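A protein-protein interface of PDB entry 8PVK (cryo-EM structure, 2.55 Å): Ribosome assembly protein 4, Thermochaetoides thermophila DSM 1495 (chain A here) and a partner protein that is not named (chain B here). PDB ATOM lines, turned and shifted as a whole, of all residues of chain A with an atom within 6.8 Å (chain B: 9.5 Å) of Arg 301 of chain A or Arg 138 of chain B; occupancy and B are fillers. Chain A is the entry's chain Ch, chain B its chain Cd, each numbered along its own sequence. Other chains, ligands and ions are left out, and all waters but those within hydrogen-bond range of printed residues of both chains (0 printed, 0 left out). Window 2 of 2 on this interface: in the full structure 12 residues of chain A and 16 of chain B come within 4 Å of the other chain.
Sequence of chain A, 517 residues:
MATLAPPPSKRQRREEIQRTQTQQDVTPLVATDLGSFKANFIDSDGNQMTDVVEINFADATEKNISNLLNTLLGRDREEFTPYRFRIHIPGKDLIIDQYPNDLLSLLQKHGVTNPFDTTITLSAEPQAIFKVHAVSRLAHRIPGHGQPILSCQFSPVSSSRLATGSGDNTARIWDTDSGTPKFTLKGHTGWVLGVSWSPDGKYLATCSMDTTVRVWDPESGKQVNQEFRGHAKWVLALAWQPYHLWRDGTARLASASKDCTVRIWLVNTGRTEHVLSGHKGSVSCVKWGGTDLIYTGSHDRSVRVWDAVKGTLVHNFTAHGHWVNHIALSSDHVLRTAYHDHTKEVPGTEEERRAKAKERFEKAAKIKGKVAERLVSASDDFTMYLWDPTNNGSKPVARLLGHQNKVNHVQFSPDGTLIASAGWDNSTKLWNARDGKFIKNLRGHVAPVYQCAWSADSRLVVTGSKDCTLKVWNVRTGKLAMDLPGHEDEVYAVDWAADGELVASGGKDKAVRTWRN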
ATOM      1  N   LYS A 280     -21.674  14.697 -15.471  1.00  0.00           N
ATOM      2  CA  LYS A 280     -20.411  14.117 -15.906  1.00  0.00           C
ATOM      3  C   LYS A 280     -19.198  14.866 -15.373  1.00  0.00           C
ATOM      4  O   LYS A 280     -18.073  14.378 -15.522  1.00  0.00           O
ATOM      5  CB  LYS A 280     -20.348  14.069 -17.437  1.00  0.00           C
ATOM      6  CG  LYS A 280     -21.366  13.136 -18.063  1.00  0.00           C
ATOM      7  CD  LYS A 280     -21.149  13.009 -19.560  1.00  0.00           C
ATOM      8  CE  LYS A 280     -21.619  14.255 -20.290  1.00  0.00           C
ATOM      9  NZ  LYS A 280     -21.539  14.093 -21.767  1.00  0.00           N
ATOM     10  N   SER A 298     -22.809  22.445 -13.227  1.00  0.00           N
ATOM     11  CA  SER A 298     -21.656  21.554 -13.205  1.00  0.00           C
ATOM     12  C   SER A 298     -20.660  21.916 -14.297  1.00  0.00           C
ATOM     13  O   SER A 298     -20.932  22.726 -15.186  1.00  0.00           O
ATOM     14  CB  SER A 298     -22.079  20.091 -13.341  1.00  0.00           C
ATOM     15  OG  SER A 298     -20.954  19.250 -13.511  1.00  0.00           O
ATOM     16  N   HIS A 299     -19.485  21.286 -14.207  1.00  0.00           N
ATOM     17  CA  HIS A 299     -18.400  21.481 -15.161  1.00  0.00           C
ATOM     18  C   HIS A 299     -18.632  20.757 -16.480  1.00  0.00           C
ATOM     19  O   HIS A 299     -17.827  20.923 -17.403  1.00  0.00           O
ATOM     20  CB  HIS A 299     -17.077  21.019 -14.552  1.00  0.00           C
ATOM     21  CG  HIS A 299     -16.469  22.011 -13.609  1.00  0.00           C
ATOM     22  ND1 HIS A 299     -15.215  21.846 -13.063  1.00  0.00           N
ATOM     23  CD2 HIS A 299     -16.942  23.181 -13.119  1.00  0.00           C
ATOM     24  CE1 HIS A 299     -14.942  22.870 -12.275  1.00  0.00           C
ATOM     25  NE2 HIS A 299     -15.974  23.694 -12.291  1.00  0.00           N
ATOM     26  N   ASP A 300     -19.694  19.961 -16.596  1.00  0.00           N
ATOM     27  CA  ASP A 300     -20.070  19.350 -17.862  1.00  0.00           C
ATOM     28  C   ASP A 300     -20.988  20.245 -18.693  1.00  0.00           C
ATOM     29  O   ASP A 300     -21.796  19.727 -19.475  1.00  0.00           O
ATOM     30  CB  ASP A 300     -20.697  17.969 -17.625  1.00  0.00           C
ATOM     31  CG  ASP A 300     -22.015  18.018 -16.856  1.00  0.00           C
ATOM     32  OD1 ASP A 300     -22.430  19.095 -16.385  1.00  0.00           O
ATOM     33  OD2 ASP A 300     -22.648  16.952 -16.723  1.00  0.00           O
ATOM     34  N   ARG A 301     -20.889  21.567 -18.507  1.00  0.00           N
ATOM     35  CA  ARG A 301     -21.611  22.586 -19.274  1.00  0.00           C
ATOM     36  C   ARG A 301     -23.124  22.479 -19.099  1.00  0.00           C
ATOM     37  O   ARG A 301     -23.882  22.827 -20.005  1.00  0.00           O
ATOM     38  CB  ARG A 301     -21.244  22.536 -20.764  1.00  0.00           C
ATOM     39  CG  ARG A 301     -19.749  22.465 -21.039  1.00  0.00           C
ATOM     40  CD  ARG A 301     -19.462  22.303 -22.518  1.00  0.00           C
ATOM     41  NE  ARG A 301     -20.093  21.107 -23.063  1.00  0.00           N
ATOM     42  CZ  ARG A 301     -19.567  19.892 -23.006  1.00  0.00           C
ATOM     43  NH1 ARG A 301     -18.396  19.670 -22.430  1.00  0.00           N
ATOM     44  NH2 ARG A 301     -20.233  18.872 -23.539  1.00  0.00           N
ATOM     45  N   SER A 302     -23.582  22.014 -17.939  1.00  0.00           N
ATOM     46  CA  SER A 302     -24.993  21.730 -17.738  1.00  0.00           C
ATOM     47  C   SER A 302     -25.519  22.389 -16.469  1.00  0.00           C
ATOM     48  O   SER A 302     -24.796  22.559 -15.475  1.00  0.00           O
ATOM     49  CB  SER A 302     -25.257  20.221 -17.680  1.00  0.00           C
ATOM     50  OG  SER A 302     -24.689  19.648 -16.517  1.00  0.00           O
ATOM     51  N   VAL A 303     -26.797  22.763 -16.534  1.00  0.00           N
ATOM     52  CA  VAL A 303     -27.556  23.289 -15.405  1.00  0.00           C
ATOM     53  C   VAL A 303     -28.806  22.432 -15.261  1.00  0.00           C
ATOM     54  O   VAL A 303     -29.611  22.342 -16.193  1.00  0.00           O
ATOM     55  CB  VAL A 303     -27.934  24.767 -15.600  1.00  0.00           C
ATOM     56  CG1 VAL A 303     -28.854  25.231 -14.485  1.00  0.00           C
ATOM     57  CG2 VAL A 303     -26.688  25.634 -15.664  1.00  0.00           C
ATOM     58  N   ASN A 316     -33.056  19.647 -17.568  1.00  0.00           N
ATOM     59  CA  ASN A 316     -31.635  19.568 -17.902  1.00  0.00           C
ATOM     60  C   ASN A 316     -31.366  20.539 -19.044  1.00  0.00           C
ATOM     61  O   ASN A 316     -31.868  20.342 -20.154  1.00  0.00           O
ATOM     62  CB  ASN A 316     -31.239  18.143 -18.289  1.00  0.00           C
ATOM     63  CG  ASN A 316     -29.736  17.943 -18.334  1.00  0.00           C
ATOM     64  OD1 ASN A 316     -28.963  18.867 -18.088  1.00  0.00           O
ATOM     65  ND2 ASN A 316     -29.313  16.726 -18.655  1.00  0.00           N
ATOM     66  N   PHE A 317     -30.577  21.578 -18.779  1.00  0.00           N
ATOM     67  CA  PHE A 317     -30.221  22.577 -19.776  1.00  0.00           C
ATOM     68  C   PHE A 317     -28.748  22.424 -20.126  1.00  0.00           C
ATOM     69  O   PHE A 317     -27.893  22.395 -19.232  1.00  0.00           O
ATOM     70  CB  PHE A 317     -30.484  23.995 -19.264  1.00  0.00           C
ATOM     71  CG  PHE A 317     -31.790  24.160 -18.534  1.00  0.00           C
ATOM     72  CD1 PHE A 317     -32.972  23.653 -19.051  1.00  0.00           C
ATOM     73  CD2 PHE A 317     -31.831  24.838 -17.327  1.00  0.00           C
ATOM     74  CE1 PHE A 317     -34.164  23.812 -18.370  1.00  0.00           C
ATOM     75  CE2 PHE A 317     -33.021  25.002 -16.646  1.00  0.00           C
ATOM     76  CZ  PHE A 317     -34.188  24.490 -17.169  1.00  0.00           C
ATOM     77  N   THR A 318     -28.456  22.335 -21.420  1.00  0.00           N
ATOM     78  CA  THR A 318     -27.105  22.133 -21.935  1.00  0.00           C
ATOM     79  C   THR A 318     -26.761  23.206 -22.960  1.00  0.00           C
ATOM     80  O   THR A 318     -26.258  22.926 -24.050  1.00  0.00           O
ATOM     81  CB  THR A 318     -26.950  20.744 -22.551  1.00  0.00           C
ATOM     82  OG1 THR A 318     -28.004  20.518 -23.495  1.00  0.00           O
ATOM     83  CG2 THR A 318     -26.995  19.669 -21.476  1.00  0.00           C
ATOM     84  N   ALA A 319     -27.037  24.463 -22.618  1.00  0.00           N
ATOM     85  CA  ALA A 319     -26.803  25.565 -23.542  1.00  0.00           C
ATOM     86  C   ALA A 319     -25.410  26.168 -23.417  1.00  0.00           C
ATOM     87  O   ALA A 319     -24.920  26.769 -24.380  1.00  0.00           O
ATOM     88  CB  ALA A 319     -27.849  26.662 -23.331  1.00  0.00           C
ATOM     89  N   HIS A 320     -24.764  26.028 -22.263  1.00  0.00           N
ATOM     90  CA  HIS A 320     -23.458  26.638 -22.061  1.00  0.00           C
ATOM     91  C   HIS A 320     -22.377  25.887 -22.832  1.00  0.00           C
ATOM     92  O   HIS A 320     -22.477  24.682 -23.077  1.00  0.00           O
ATOM     93  CB  HIS A 320     -23.108  26.675 -20.575  1.00  0.00           C
ATOM     94  CG  HIS A 320     -23.875  27.700 -19.799  1.00  0.00           C
ATOM     95  ND1 HIS A 320     -23.715  29.054 -19.993  1.00  0.00           N
ATOM     96  CD2 HIS A 320     -24.804  27.567 -18.823  1.00  0.00           C
ATOM     97  CE1 HIS A 320     -24.507  29.713 -19.167  1.00  0.00           C
ATOM     98  NE2 HIS A 320     -25.184  28.834 -18.450  1.00  0.00           N
ATOM     99  N   GLY A 321     -21.334  26.618 -23.215  1.00  0.00           N
ATOM    100  CA  GLY A 321     -20.240  26.080 -23.988  1.00  0.00           C
ATOM    101  C   GLY A 321     -18.989  25.723 -23.219  1.00  0.00           C
ATOM    102  O   GLY A 321     -18.062  25.160 -23.807  1.00  0.00           O
ATOM    103  N   HIS A 322     -18.925  26.031 -21.926  1.00  0.00           N
ATOM    104  CA  HIS A 322     -17.791  25.643 -21.097  1.00  0.00           C
ATOM    105  C   HIS A 322     -18.322  25.445 -19.678  1.00  0.00           C
ATOM    106  O   HIS A 322     -19.530  25.289 -19.474  1.00  0.00           O
ATOM    107  CB  HIS A 322     -16.669  26.685 -21.208  1.00  0.00           C
ATOM    108  CG  HIS A 322     -15.295  26.136 -20.952  1.00  0.00           C
ATOM    109  ND1 HIS A 322     -14.736  26.055 -19.695  1.00  0.00           N
ATOM    110  CD2 HIS A 322     -14.368  25.641 -21.805  1.00  0.00           C
ATOM    111  CE1 HIS A 322     -13.526  25.534 -19.783  1.00  0.00           C
ATOM    112  NE2 HIS A 322     -13.278  25.273 -21.053  1.00  0.00           N
ATOM    113  N   TRP A 323     -17.414  25.434 -18.699  1.00  0.00           N
ATOM    114  CA  TRP A 323     -17.768  25.183 -17.305  1.00  0.00           C
ATOM    115  C   TRP A 323     -18.773  26.201 -16.786  1.00  0.00           C
ATOM    116  O   TRP A 323     -18.604  27.408 -16.966  1.00  0.00           O
ATOM    117  CB  TRP A 323     -16.527  25.253 -16.415  1.00  0.00           C
ATOM    118  CG  TRP A 323     -15.518  24.180 -16.596  1.00  0.00           C
ATOM    119  CD1 TRP A 323     -15.572  23.127 -17.457  1.00  0.00           C
ATOM    120  CD2 TRP A 323     -14.286  24.054 -15.883  1.00  0.00           C
ATOM    121  NE1 TRP A 323     -14.446  22.352 -17.325  1.00  0.00           N
ATOM    122  CE2 TRP A 323     -13.640  22.901 -16.363  1.00  0.00           C
ATOM    123  CE3 TRP A 323     -13.666  24.808 -14.880  1.00  0.00           C
ATOM    124  CZ2 TRP A 323     -12.404  22.483 -15.878  1.00  0.00           C
ATOM    125  CZ3 TRP A 323     -12.442  24.393 -14.401  1.00  0.00           C
ATOM    126  CH2 TRP A 323     -11.823  23.241 -14.900  1.00  0.00           C
ATOM    127  N   VAL A 324     -19.813  25.709 -16.121  1.00  0.00           N
ATOM    128  CA  VAL A 324     -20.732  26.581 -15.401  1.00  0.00           C
ATOM    129  C   VAL A 324     -20.083  26.955 -14.076  1.00  0.00           C
ATOM    130  O   VAL A 324     -19.805  26.088 -13.243  1.00  0.00           O
ATOM    131  CB  VAL A 324     -22.091  25.902 -15.182  1.00  0.00           C
ATOM    132  CG1 VAL A 324     -22.939  26.715 -14.218  1.00  0.00           C
ATOM    133  CG2 VAL A 324     -22.811  25.724 -16.505  1.00  0.00           C
ATOM    134  N   ASP A 381     -17.867  30.198 -20.756  1.00  0.00           N
ATOM    135  CA  ASP A 381     -17.963  30.542 -22.166  1.00  0.00           C
ATOM    136  C   ASP A 381     -18.256  32.023 -22.387  1.00  0.00           C
ATOM    137  O   ASP A 381     -18.844  32.379 -23.414  1.00  0.00           O
ATOM    138  CB  ASP A 381     -19.004  29.661 -22.870  1.00  0.00           C
ATOM    139  CG  ASP A 381     -20.403  29.780 -22.279  1.00  0.00           C
ATOM    140  OD1 ASP A 381     -20.657  30.632 -21.403  1.00  0.00           O
ATOM    141  OD2 ASP A 381     -21.277  29.011 -22.721  1.00  0.00           O
ATOM    142  N   LEU B 127     -15.437  37.272 -28.468  1.00  0.00           N
ATOM    143  CA  LEU B 127     -15.819  35.865 -28.553  1.00  0.00           C
ATOM    144  C   LEU B 127     -15.076  35.153 -29.680  1.00  0.00           C
ATOM    145  O   LEU B 127     -14.711  33.977 -29.544  1.00  0.00           O
ATOM    146  CB  LEU B 127     -17.330  35.742 -28.742  1.00  0.00           C
ATOM    147  CG  LEU B 127     -18.194  36.169 -27.554  1.00  0.00           C
ATOM    148  CD1 LEU B 127     -19.665  36.160 -27.931  1.00  0.00           C
ATOM    149  CD2 LEU B 127     -17.941  35.269 -26.357  1.00  0.00           C
ATOM    150  N   HIS B 130     -11.559  33.807 -29.020  1.00  0.00           N
ATOM    151  CA  HIS B 130     -11.451  32.691 -28.095  1.00  0.00           C
ATOM    152  C   HIS B 130     -12.293  31.481 -28.476  1.00  0.00           C
ATOM    153  O   HIS B 130     -12.266  30.487 -27.744  1.00  0.00           O
ATOM    154  CB  HIS B 130     -11.832  33.140 -26.678  1.00  0.00           C
ATOM    155  CG  HIS B 130     -10.924  34.187 -26.114  1.00  0.00           C
ATOM    156  ND1 HIS B 130     -11.154  35.537 -26.273  1.00  0.00           N
ATOM    157  CD2 HIS B 130      -9.783  34.083 -25.393  1.00  0.00           C
ATOM    158  CE1 HIS B 130     -10.195  36.218 -25.674  1.00  0.00           C
ATOM    159  NE2 HIS B 130      -9.350  35.360 -25.131  1.00  0.00           N
ATOM    160  N   GLN B 131     -13.042  31.540 -29.587  1.00  0.00           N
ATOM    161  CA  GLN B 131     -13.870  30.403 -29.995  1.00  0.00           C
ATOM    162  C   GLN B 131     -13.047  29.145 -30.261  1.00  0.00           C
ATOM    163  O   GLN B 131     -13.444  28.046 -29.858  1.00  0.00           O
ATOM    164  CB  GLN B 131     -14.686  30.759 -31.237  1.00  0.00           C
ATOM    165  CG  GLN B 131     -16.032  31.392 -30.948  1.00  0.00           C
ATOM    166  CD  GLN B 131     -16.862  30.572 -29.983  1.00  0.00           C
ATOM    167  OE1 GLN B 131     -17.075  30.970 -28.838  1.00  0.00           O
ATOM    168  NE2 GLN B 131     -17.335  29.420 -30.440  1.00  0.00           N
ATOM    169  N   ALA B 132     -11.905  29.282 -30.940  1.00  0.00           N
ATOM    170  CA  ALA B 132     -11.098  28.113 -31.286  1.00  0.00           C
ATOM    171  C   ALA B 132     -10.515  27.450 -30.042  1.00  0.00           C
ATOM    172  O   ALA B 132     -10.602  26.224 -29.877  1.00  0.00           O
ATOM    173  CB  ALA B 132      -9.985  28.516 -32.252  1.00  0.00           C
ATOM    174  N   LYS B 133      -9.930  28.253 -29.148  1.00  0.00           N
ATOM    175  CA  LYS B 133      -9.403  27.728 -27.893  1.00  0.00           C
ATOM    176  C   LYS B 133     -10.507  27.139 -27.028  1.00  0.00           C
ATOM    177  O   LYS B 133     -10.290  26.131 -26.348  1.00  0.00           O
ATOM    178  CB  LYS B 133      -8.665  28.832 -27.136  1.00  0.00           C
ATOM    179  CG  LYS B 133      -7.875  28.347 -25.934  1.00  0.00           C
ATOM    180  CD  LYS B 133      -7.107  29.485 -25.286  1.00  0.00           C
ATOM    181  CE  LYS B 133      -6.266  28.989 -24.124  1.00  0.00           C
ATOM    182  NZ  LYS B 133      -7.111  28.537 -22.985  1.00  0.00           N
ATOM    183  N   MET B 134     -11.701  27.734 -27.066  1.00  0.00           N
ATOM    184  CA  MET B 134     -12.826  27.227 -26.292  1.00  0.00           C
ATOM    185  C   MET B 134     -13.288  25.869 -26.808  1.00  0.00           C
ATOM    186  O   MET B 134     -13.581  24.966 -26.017  1.00  0.00           O
ATOM    187  CB  MET B 134     -13.958  28.248 -26.344  1.00  0.00           C
ATOM    188  CG  MET B 134     -15.163  27.948 -25.492  1.00  0.00           C
ATOM    189  SD  MET B 134     -16.339  29.289 -25.715  1.00  0.00           S
ATOM    190  CE  MET B 134     -15.486  30.593 -24.830  1.00  0.00           C
ATOM    191  N   THR B 135     -13.341  25.701 -28.133  1.00  0.00           N
ATOM    192  CA  THR B 135     -13.726  24.411 -28.702  1.00  0.00           C
ATOM    193  C   THR B 135     -12.672  23.345 -28.427  1.00  0.00           C
ATOM    194  O   THR B 135     -13.015  22.184 -28.177  1.00  0.00           O
ATOM    195  CB  THR B 135     -13.974  24.534 -30.206  1.00  0.00           C
ATOM    196  OG1 THR B 135     -12.826  25.107 -30.842  1.00  0.00           O
ATOM    197  CG2 THR B 135     -15.201  25.388 -30.482  1.00  0.00           C
ATOM    198  N   ILE B 136     -11.389  23.717 -28.466  1.00  0.00           N
ATOM    199  CA  ILE B 136     -10.339  22.746 -28.163  1.00  0.00           C
ATOM    200  C   ILE B 136     -10.370  22.358 -26.686  1.00  0.00           C
ATOM    201  O   ILE B 136     -10.156  21.190 -26.333  1.00  0.00           O
ATOM    202  CB  ILE B 136      -8.965  23.292 -28.597  1.00  0.00           C
ATOM    203  CG1 ILE B 136      -8.933  23.483 -30.112  1.00  0.00           C
ATOM    204  CG2 ILE B 136      -7.836  22.356 -28.191  1.00  0.00           C
ATOM    205  CD1 ILE B 136      -9.384  22.268 -30.890  1.00  0.00           C
ATOM    206  N   GLU B 137     -10.659  23.318 -25.803  1.00  0.00           N
ATOM    207  CA  GLU B 137     -10.792  23.008 -24.381  1.00  0.00           C
ATOM    208  C   GLU B 137     -12.006  22.127 -24.115  1.00  0.00           C
ATOM    209  O   GLU B 137     -11.965  21.255 -23.239  1.00  0.00           O
ATOM    210  CB  GLU B 137     -10.885  24.299 -23.570  1.00  0.00           C
ATOM    211  CG  GLU B 137      -9.548  24.959 -23.290  1.00  0.00           C
ATOM    212  CD  GLU B 137      -9.697  26.305 -22.610  1.00  0.00           C
ATOM    213  OE1 GLU B 137     -10.821  26.848 -22.605  1.00  0.00           O
ATOM    214  OE2 GLU B 137      -8.690  26.819 -22.081  1.00  0.00           O
ATOM    215  N   ARG B 138     -13.098  22.352 -24.847  1.00  0.00           N
ATOM    216  CA  ARG B 138     -14.293  21.533 -24.678  1.00  0.00           C
ATOM    217  C   ARG B 138     -14.065  20.110 -25.175  1.00  0.00           C
ATOM    218  O   ARG B 138     -14.381  19.140 -24.478  1.00  0.00           O
ATOM    219  CB  ARG B 138     -15.469  22.182 -25.406  1.00  0.00           C
ATOM    220  CG  ARG B 138     -16.810  21.519 -25.166  1.00  0.00           C
ATOM    221  CD  ARG B 138     -17.859  22.025 -26.147  1.00  0.00           C
ATOM    222  NE  ARG B 138     -17.799  23.470 -26.330  1.00  0.00           N
ATOM    223  CZ  ARG B 138     -17.519  24.070 -27.479  1.00  0.00           C
ATOM    224  NH1 ARG B 138     -17.269  23.376 -28.577  1.00  0.00           N
ATOM    225  NH2 ARG B 138     -17.489  25.397 -27.527  1.00  0.00           N
ATOM    226  N   GLU B 139     -13.518  19.965 -26.377  1.00  0.00           N
ATOM    227  CA  GLU B 139     -13.189  18.656 -26.940  1.00  0.00           C
ATOM    228  C   GLU B 139     -11.769  18.688 -27.483  1.00  0.00           C
ATOM    229  O   GLU B 139     -11.503  19.413 -28.464  1.00  0.00           O
ATOM    230  CB  GLU B 139     -14.168  18.258 -28.042  1.00  0.00           C
ATOM    231  CG  GLU B 139     -15.586  17.994 -27.571  1.00  0.00           C
ATOM    232  CD  GLU B 139     -16.543  19.106 -27.945  1.00  0.00           C
ATOM    233  OE1 GLU B 139     -16.123  20.042 -28.658  1.00  0.00           O
ATOM    234  OE2 GLU B 139     -17.720  19.037 -27.535  1.00  0.00           O
ATOM    235  N   PRO B 140     -10.836  17.949 -26.890  1.00  0.00           N
ATOM    236  CA  PRO B 140      -9.491  17.854 -27.468  1.00  0.00           C
ATOM    237  C   PRO B 140      -9.499  17.098 -28.788  1.00  0.00           C
ATOM    238  O   PRO B 140     -10.474  16.439 -29.159  1.00  0.00           O
ATOM    239  CB  PRO B 140      -8.684  17.100 -26.404  1.00  0.00           C
ATOM    240  CG  PRO B 140      -9.680  16.551 -25.447  1.00  0.00           C
ATOM    241  CD  PRO B 140     -10.898  17.402 -25.526  1.00  0.00           C
ATOM    242  N   PHE B 141      -8.378  17.218 -29.506  1.00  0.00           N
ATOM    243  CA  PHE B 141      -8.254  16.603 -30.824  1.00  0.00           C
ATOM    244  C   PHE B 141      -8.311  15.081 -30.743  1.00  0.00           C
ATOM    245  O   PHE B 141      -8.875  14.426 -31.627  1.00  0.00           O
ATOM    246  CB  PHE B 141      -6.950  17.046 -31.488  1.00  0.00           C
ATOM    247  CG  PHE B 141      -7.022  18.398 -32.136  1.00  0.00           C
ATOM    248  CD1 PHE B 141      -7.776  18.595 -33.281  1.00  0.00           C
ATOM    249  CD2 PHE B 141      -6.323  19.470 -31.609  1.00  0.00           C
ATOM    250  CE1 PHE B 141      -7.838  19.836 -33.882  1.00  0.00           C
ATOM    251  CE2 PHE B 141      -6.379  20.714 -32.205  1.00  0.00           C
ATOM    252  CZ  PHE B 141      -7.136  20.896 -33.344  1.00  0.00           C
ATOM    253  N   GLU B 143      -9.937  13.155 -28.659  1.00  0.00           N
ATOM    254  CA  GLU B 143     -11.274  12.642 -28.391  1.00  0.00           C
ATOM    255  C   GLU B 143     -12.238  12.856 -29.548  1.00  0.00           C
ATOM    256  O   GLU B 143     -13.366  12.357 -29.494  1.00  0.00           O
ATOM    257  CB  GLU B 143     -11.849  13.291 -27.128  1.00  0.00           C
ATOM    258  CG  GLU B 143     -11.002  13.092 -25.887  1.00  0.00           C
ATOM    259  CD  GLU B 143     -11.630  13.709 -24.653  1.00  0.00           C
ATOM    260  OE1 GLU B 143     -12.756  14.238 -24.760  1.00  0.00           O
ATOM    261  OE2 GLU B 143     -10.995  13.669 -23.579  1.00  0.00           O
ATOM    262  N   THR B 144     -11.826  13.580 -30.585  1.00  0.00           N
ATOM    263  CA  THR B 144     -12.678  13.872 -31.730  1.00  0.00           C
ATOM    264  C   THR B 144     -12.489  12.878 -32.867  1.00  0.00           C
ATOM    265  O   THR B 144     -13.457  12.256 -33.315  1.00  0.00           O
ATOM    266  CB  THR B 144     -12.406  15.295 -32.230  1.00  0.00           C
ATOM    267  OG1 THR B 144     -12.664  16.230 -31.177  1.00  0.00           O
ATOM    268  CG2 THR B 144     -13.289  15.613 -33.411  1.00  0.00           C
ATOM    269  N   ARG B 153     -21.824  12.023 -31.128  1.00  0.00           N
ATOM    270  CA  ARG B 153     -22.866  12.907 -31.627  1.00  0.00           C
ATOM    271  C   ARG B 153     -22.236  14.064 -32.383  1.00  0.00           C
ATOM    272  O   ARG B 153     -21.418  14.796 -31.806  1.00  0.00           O
ATOM    273  CB  ARG B 153     -23.719  13.429 -30.473  1.00  0.00           C
ATOM    274  CG  ARG B 153     -24.401  12.342 -29.667  1.00  0.00           C
ATOM    275  CD  ARG B 153     -25.507  11.675 -30.460  1.00  0.00           C
ATOM    276  NE  ARG B 153     -26.150  10.611 -29.699  1.00  0.00           N
ATOM    277  CZ  ARG B 153     -27.170  10.794 -28.873  1.00  0.00           C
ATOM    278  NH1 ARG B 153     -27.678  11.997 -28.657  1.00  0.00           N
ATOM    279  NH2 ARG B 153     -27.690   9.745 -28.242  1.00  0.00           N
ATOM    280  N   LYS B 155     -22.070  17.804 -34.450  1.00  0.00           N
ATOM    281  CA  LYS B 155     -22.604  19.144 -34.243  1.00  0.00           C
ATOM    282  C   LYS B 155     -23.304  19.589 -35.520  1.00  0.00           C
ATOM    283  O   LYS B 155     -22.672  19.682 -36.577  1.00  0.00           O
ATOM    284  CB  LYS B 155     -21.492  20.121 -33.862  1.00  0.00           C
ATOM    285  CG  LYS B 155     -21.975  21.528 -33.563  1.00  0.00           C
ATOM    286  CD  LYS B 155     -20.807  22.453 -33.260  1.00  0.00           C
ATOM    287  CE  LYS B 155     -21.258  23.899 -33.149  1.00  0.00           C
ATOM    288  NZ  LYS B 155     -21.881  24.386 -34.411  1.00  0.00           N
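OE1 of Glu 137 of chain B is in hydrogen-bond range of NE2 of His 322 of chain A, at 3.3 Å. The backbone carbonyl oxygen (O) of Gly 321 of chain A lies within hydrogen-bond range of the guanidinium group (NE) of Arg 138 of chain B (3.0 Å).
The side-chain sulfur (SD) of Met 134 of chain B lies close to the side-chain amide oxygen (OE1) of Gln 131 of chain B (3.6 Å). NZ of Lys 133 of chain B lies within salt-bridge range of OE2 of Glu 137 of chain B (2.5 Å). The backbone NH (N) of Gly 321 of chain A is in hydrogen-bond range of the side-chain carboxylate (OD2) of Asp 381 of chain A, at 2.4 Å. NH1 of Arg 138 of chain B lies within salt-bridge range of OE1 of Glu 139 of chain B.
Among the printed residues, pairs that only touch across the chains: Asp 381 of chain A with Met 134 of chain B and Arg 301 of chain A with Arg 138 of chain B.
Arg 301 of chain A touches just one residue of chain B: Arg 138. Arg 138 of chain B touches two residues of chain A. Asp 300 of chain A touches none of the printed residues of chain B. Of the printed residues of chain A, Met 134 of chain B touches Asp 381. Of the printed residues of chain A, Glu 137 of chain B touches His 322 (3.3 Å). Of the printed residues of chain B, His 322 of chain A touches Glu 137 (3.3 Å). Of the printed residues of chain B, Asp 381 of chain A touches Met 134 (3.6 Å). The nearest printed residue of chain B that does not touch Asp 381 of chain A is Leu 127 of chain B (4.2 Å).
Of the 17 printed residues of chain A, 4 touch a printed residue of chain B. Hydrophobic or aromatic side chains of chain A that line the printed part of chain B: His 322. Of the 17 printed residues of chain B, 3 touch a printed residue of chain A. Printed residues of chain B that touch a printed residue of chain A: Met 134, Glu 137 and Arg 138. Hydrophobic or aromatic side chains of chain B that line the printed part of chain A: Met 134. Among the printed residues, no Asp or Glu carboxylate lies within 4 Å of a Lys or Arg side-chain nitrogen of the other chain.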
